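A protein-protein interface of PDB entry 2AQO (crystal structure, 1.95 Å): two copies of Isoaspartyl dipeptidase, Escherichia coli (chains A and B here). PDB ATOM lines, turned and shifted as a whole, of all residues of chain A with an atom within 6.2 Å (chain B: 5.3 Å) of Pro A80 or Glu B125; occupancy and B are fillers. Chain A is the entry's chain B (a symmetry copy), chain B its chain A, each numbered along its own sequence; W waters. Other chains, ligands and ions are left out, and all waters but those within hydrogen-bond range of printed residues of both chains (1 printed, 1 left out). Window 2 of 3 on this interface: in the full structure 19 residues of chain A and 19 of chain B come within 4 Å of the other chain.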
ATOM      1  N   GLY A  76     -27.549 -14.109  -0.441  1.00  0.00           N
ATOM      2  CA  GLY A  76     -27.078 -13.674  -1.762  1.00  0.00           C
ATOM      3  C   GLY A  76     -28.054 -12.747  -2.502  1.00  0.00           C
ATOM      4  O   GLY A  76     -27.770 -12.308  -3.613  1.00  0.00           O
ATOM      5  N   ALA A  78     -28.840  -9.753  -1.806  1.00  0.00           N
ATOM      6  CA  ALA A  78     -28.397  -8.371  -1.900  1.00  0.00           C
ATOM      7  C   ALA A  78     -26.923  -8.397  -2.278  1.00  0.00           C
ATOM      8  O   ALA A  78     -26.068  -7.730  -1.712  1.00  0.00           O
ATOM      9  CB  ALA A  78     -28.680  -7.618  -0.621  1.00  0.00           C
ATOM     10  N   GLY A  79     -26.606  -9.252  -3.241  1.00  0.00           N
ATOM     11  CA  GLY A  79     -25.219  -9.342  -3.637  1.00  0.00           C
ATOM     12  C   GLY A  79     -24.422 -10.322  -2.820  1.00  0.00           C
ATOM     13  O   GLY A  79     -24.832 -10.779  -1.769  1.00  0.00           O
ATOM     14  N   PRO A  80     -23.224 -10.590  -3.350  1.00  0.00           N
ATOM     15  CA  PRO A  80     -22.239 -11.554  -2.903  1.00  0.00           C
ATOM     16  C   PRO A  80     -21.885 -11.611  -1.429  1.00  0.00           C
ATOM     17  O   PRO A  80     -21.652 -12.692  -0.865  1.00  0.00           O
ATOM     18  CB  PRO A  80     -21.014 -11.420  -3.800  1.00  0.00           C
ATOM     19  CG  PRO A  80     -21.453 -10.545  -4.960  1.00  0.00           C
ATOM     20  CD  PRO A  80     -22.731  -9.843  -4.533  1.00  0.00           C
ATOM     21  N   THR A  81     -21.850 -10.454  -0.808  1.00  0.00           N
ATOM     22  CA  THR A  81     -21.516 -10.403   0.608  1.00  0.00           C
ATOM     23  C   THR A  81     -22.631 -10.992   1.469  1.00  0.00           C
ATOM     24  O   THR A  81     -22.401 -11.374   2.621  1.00  0.00           O
ATOM     25  CB  THR A  81     -21.243  -8.964   1.059  1.00  0.00           C
ATOM     26  OG1 THR A  81     -22.463  -8.273   0.912  1.00  0.00           O
ATOM     27  CG2 THR A  81     -20.188  -8.272   0.189  1.00  0.00           C
ATOM     28  N   THR A  82     -23.855 -11.080   0.917  1.00  0.00           N
ATOM     29  CA  THR A  82     -24.945 -11.629   1.690  1.00  0.00           C
ATOM     30  C   THR A  82     -25.072 -13.131   1.647  1.00  0.00           C
ATOM     31  O   THR A  82     -26.073 -13.687   2.130  1.00  0.00           O
ATOM     32  CB  THR A  82     -26.286 -10.930   1.415  1.00  0.00           C
ATOM     33  OG1 THR A  82     -26.774 -11.222   0.097  1.00  0.00           O
ATOM     34  CG2 THR A  82     -26.012  -9.445   1.581  1.00  0.00           C
ATOM     35  N   ARG A  83     -24.072 -13.806   1.092  1.00  0.00           N
ATOM     36  CA  ARG A  83     -24.134 -15.281   1.082  1.00  0.00           C
ATOM     37  C   ARG A  83     -23.778 -15.804   2.473  1.00  0.00           C
ATOM     38  O   ARG A  83     -22.648 -15.589   2.943  1.00  0.00           O
ATOM     39  CB  ARG A  83     -23.108 -15.828   0.098  1.00  0.00           C
ATOM     40  CG  ARG A  83     -23.611 -15.511  -1.314  1.00  0.00           C
ATOM     41  CD  ARG A  83     -22.512 -15.693  -2.343  1.00  0.00           C
ATOM     42  NE  ARG A  83     -22.317 -17.118  -2.660  1.00  0.00           N
ATOM     43  CZ  ARG A  83     -21.338 -17.913  -2.220  1.00  0.00           C
ATOM     44  NH1 ARG A  83     -20.326 -17.487  -1.426  1.00  0.00           N
ATOM     45  NH2 ARG A  83     -21.366 -19.178  -2.605  1.00  0.00           N
ATOM     46  N   ALA B 118     -18.251 -15.812  -6.886  1.00  0.00           N
ATOM     47  CA  ALA B 118     -19.082 -14.992  -6.006  1.00  0.00           C
ATOM     48  C   ALA B 118     -18.301 -14.549  -4.771  1.00  0.00           C
ATOM     49  O   ALA B 118     -18.337 -13.382  -4.372  1.00  0.00           O
ATOM     50  CB  ALA B 118     -20.330 -15.759  -5.550  1.00  0.00           C
ATOM     51  N   THR B 120     -15.092 -14.296  -4.453  1.00  0.00           N
ATOM     52  CA  THR B 120     -14.074 -13.329  -4.879  1.00  0.00           C
ATOM     53  C   THR B 120     -14.664 -11.926  -4.872  1.00  0.00           C
ATOM     54  O   THR B 120     -14.117 -10.928  -4.353  1.00  0.00           O
ATOM     55  CB  THR B 120     -13.518 -13.753  -6.270  1.00  0.00           C
ATOM     56  OG1 THR B 120     -12.818 -14.981  -6.199  1.00  0.00           O
ATOM     57  CG2 THR B 120     -12.595 -12.702  -6.822  1.00  0.00           C
ATOM     58  N   ARG B 121     -15.849 -11.826  -5.458  1.00  0.00           N
ATOM     59  CA  ARG B 121     -16.508 -10.531  -5.498  1.00  0.00           C
ATOM     60  C   ARG B 121     -16.881 -10.014  -4.116  1.00  0.00           C
ATOM     61  O   ARG B 121     -16.736  -8.832  -3.821  1.00  0.00           O
ATOM     62  CB  ARG B 121     -17.687 -10.575  -6.434  1.00  0.00           C
ATOM     63  CG  ARG B 121     -17.185 -10.758  -7.854  1.00  0.00           C
ATOM     64  CD  ARG B 121     -18.269 -10.941  -8.915  1.00  0.00           C
ATOM     65  NE  ARG B 121     -17.745 -10.670 -10.271  1.00  0.00           N
ATOM     66  CZ  ARG B 121     -18.354 -11.120 -11.359  1.00  0.00           C
ATOM     67  NH1 ARG B 121     -19.458 -11.848 -11.243  1.00  0.00           N
ATOM     68  NH2 ARG B 121     -17.865 -10.839 -12.552  1.00  0.00           N
ATOM     69  N   ALA B 122     -17.336 -10.898  -3.242  1.00  0.00           N
ATOM     70  CA  ALA B 122     -17.715 -10.461  -1.889  1.00  0.00           C
ATOM     71  C   ALA B 122     -16.524  -9.833  -1.166  1.00  0.00           C
ATOM     72  O   ALA B 122     -16.628  -8.792  -0.493  1.00  0.00           O
ATOM     73  CB  ALA B 122     -18.230 -11.632  -1.070  1.00  0.00           C
ATOM     74  N   LEU B 123     -15.368 -10.469  -1.332  1.00  0.00           N
ATOM     75  CA  LEU B 123     -14.140  -9.979  -0.721  1.00  0.00           C
ATOM     76  C   LEU B 123     -13.742  -8.599  -1.219  1.00  0.00           C
ATOM     77  O   LEU B 123     -13.351  -7.728  -0.431  1.00  0.00           O
ATOM     78  CB  LEU B 123     -12.984 -11.012  -0.760  1.00  0.00           C
ATOM     79  CG  LEU B 123     -13.205 -12.232   0.154  1.00  0.00           C
ATOM     80  CD1 LEU B 123     -12.187 -13.323  -0.230  1.00  0.00           C
ATOM     81  CD2 LEU B 123     -13.181 -11.886   1.666  1.00  0.00           C
ATOM     82  N   ASN B 124     -13.895  -8.346  -2.526  1.00  0.00           N
ATOM     83  CA  ASN B 124     -13.593  -7.020  -3.019  1.00  0.00           C
ATOM     84  C   ASN B 124     -14.535  -6.006  -2.422  1.00  0.00           C
ATOM     85  O   ASN B 124     -14.152  -4.883  -2.089  1.00  0.00           O
ATOM     86  CB  ASN B 124     -13.762  -6.981  -4.548  1.00  0.00           C
ATOM     87  CG  ASN B 124     -12.603  -7.694  -5.211  1.00  0.00           C
ATOM     88  OD1 ASN B 124     -11.451  -7.274  -5.108  1.00  0.00           O
ATOM     89  ND2 ASN B 124     -12.891  -8.826  -5.804  1.00  0.00           N
ATOM     90  N   GLU B 125     -15.807  -6.407  -2.340  1.00  0.00           N
ATOM     91  CA  GLU B 125     -16.840  -5.551  -1.798  1.00  0.00           C
ATOM     92  C   GLU B 125     -16.580  -5.276  -0.306  1.00  0.00           C
ATOM     93  O   GLU B 125     -16.751  -4.176   0.220  1.00  0.00           O
ATOM     94  CB  GLU B 125     -18.186  -6.215  -2.039  1.00  0.00           C
ATOM     95  CG  GLU B 125     -19.186  -5.278  -2.686  1.00  0.00           C
ATOM     96  CD  GLU B 125     -20.503  -5.963  -2.773  1.00  0.00           C
ATOM     97  OE1 GLU B 125     -20.638  -7.011  -3.390  1.00  0.00           O
ATOM     98  OE2 GLU B 125     -21.416  -5.373  -2.021  1.00  0.00           O
ATOM     99  N   GLU B 126     -16.104  -6.277   0.380  1.00  0.00           N
ATOM    100  CA  GLU B 126     -15.794  -6.139   1.780  1.00  0.00           C
ATOM    101  C   GLU B 126     -14.516  -5.314   2.025  1.00  0.00           C
ATOM    102  O   GLU B 126     -14.274  -4.906   3.154  1.00  0.00           O
ATOM    103  CB  GLU B 126     -15.745  -7.476   2.504  1.00  0.00           C
ATOM    104  CG  GLU B 126     -17.161  -7.981   2.709  1.00  0.00           C
ATOM    105  CD  GLU B 126     -17.206  -9.412   3.167  1.00  0.00           C
ATOM    106  OE1 GLU B 126     -16.262 -10.155   3.124  1.00  0.00           O
ATOM    107  OE2 GLU B 126     -18.375  -9.774   3.606  1.00  0.00           O
ATOM    108  N   GLY B 127     -13.683  -5.038   1.027  1.00  0.00           N
ATOM    109  CA  GLY B 127     -12.567  -4.184   1.395  1.00  0.00           C
ATOM    110  C   GLY B 127     -11.196  -4.529   0.883  1.00  0.00           C
ATOM    111  O   GLY B 127     -10.306  -3.663   0.870  1.00  0.00           O
ATOM    112  N   ILE B 128     -11.002  -5.783   0.486  1.00  0.00           N
ATOM    113  CA  ILE B 128      -9.677  -6.155  -0.043  1.00  0.00           C
ATOM    114  C   ILE B 128      -9.683  -6.342  -1.553  1.00  0.00           C
ATOM    115  O   ILE B 128     -10.632  -5.959  -2.221  1.00  0.00           O
ATOM    116  CB  ILE B 128      -9.032  -7.313   0.683  1.00  0.00           C
ATOM    117  CG1 ILE B 128      -9.937  -8.531   0.617  1.00  0.00           C
ATOM    118  CG2 ILE B 128      -8.815  -6.933   2.149  1.00  0.00           C
ATOM    119  CD1 ILE B 128      -9.085  -9.798   0.707  1.00  0.00           C
ATOM    120  N   ARG B 371      -6.729  -0.508   0.455  1.00  0.00           N
ATOM    121  CA  ARG B 371      -7.340   0.533  -0.325  1.00  0.00           C
ATOM    122  C   ARG B 371      -7.569   1.787   0.527  1.00  0.00           C
ATOM    123  O   ARG B 371      -8.598   2.455   0.458  1.00  0.00           O
ATOM    124  CB  ARG B 371      -8.562   0.079  -1.114  1.00  0.00           C
ATOM    125  CG  ARG B 371      -8.143  -0.988  -2.119  1.00  0.00           C
ATOM    126  CD  ARG B 371      -9.235  -1.348  -3.119  1.00  0.00           C
ATOM    127  NE  ARG B 371      -9.951  -2.542  -2.693  1.00  0.00           N
ATOM    128  CZ  ARG B 371     -11.254  -2.536  -2.513  1.00  0.00           C
ATOM    129  NH1 ARG B 371     -11.968  -1.438  -2.704  1.00  0.00           N
ATOM    130  NH2 ARG B 371     -11.863  -3.641  -2.113  1.00  0.00           N
HETATM  131  O   HOH W   1     -19.526 -12.305   3.242  1.00  0.00           O
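Pro A80 touches just these residues of chain B: Ala B118 (3.4 Å), Ala B122 (3.6 Å) and Glu B125 (3.7 Å). Glu B125 touches just these residues of chain A: Pro A80 and Thr A81. Printed residues of chain A within 4 Å of Glu B126: Thr A81. Of the printed residues of chain A, Ala B118 touches Pro A80 and Arg A83. Of the printed residues of chain B, Thr A81 touches Ala B122 (3.7 Å), Glu B125 (3.6 Å) and Glu B126 (3.9 Å). Of the printed residues of chain A, Ala B122 touches Pro A80 and Thr A81. Thr B120 touches none of the printed residues of chain A. Leu B123 touches none of the printed residues of chain A. The nearest residue of chain B that does not touch Pro A80 is Arg B121 (4.04 Å).
Among the printed residues, pairs that only touch across the chains: Pro A80 with Ala B118 (3.4 Å), Pro A80 with Ala B122 (3.6 Å), Pro A80 with Glu B125 (3.7 Å), Thr A81 with Ala B122 (3.7 Å), Thr A81 with Glu B125 (3.6 Å), Thr A81 with Glu B126 (3.9 Å) and Arg A83 with Ala B118 (3.8 Å).
Of the 11 printed residues of chain B, 4 touch a printed residue of chain A. Printed residues of chain B that touch a printed residue of chain A: Ala B118, Ala B122, Glu B125 and Glu B126. Hydrophobic or aromatic side chains of chain A within 4 Å of the printed part of chain B: Pro A80.
No position is printed for both chains.
Water W1 lies within hydrogen-bond range of the side-chain carboxylate of Glu B126 (2.8 Å) and the backbone carbonyl oxygen of Thr A81 (3.1 Å).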
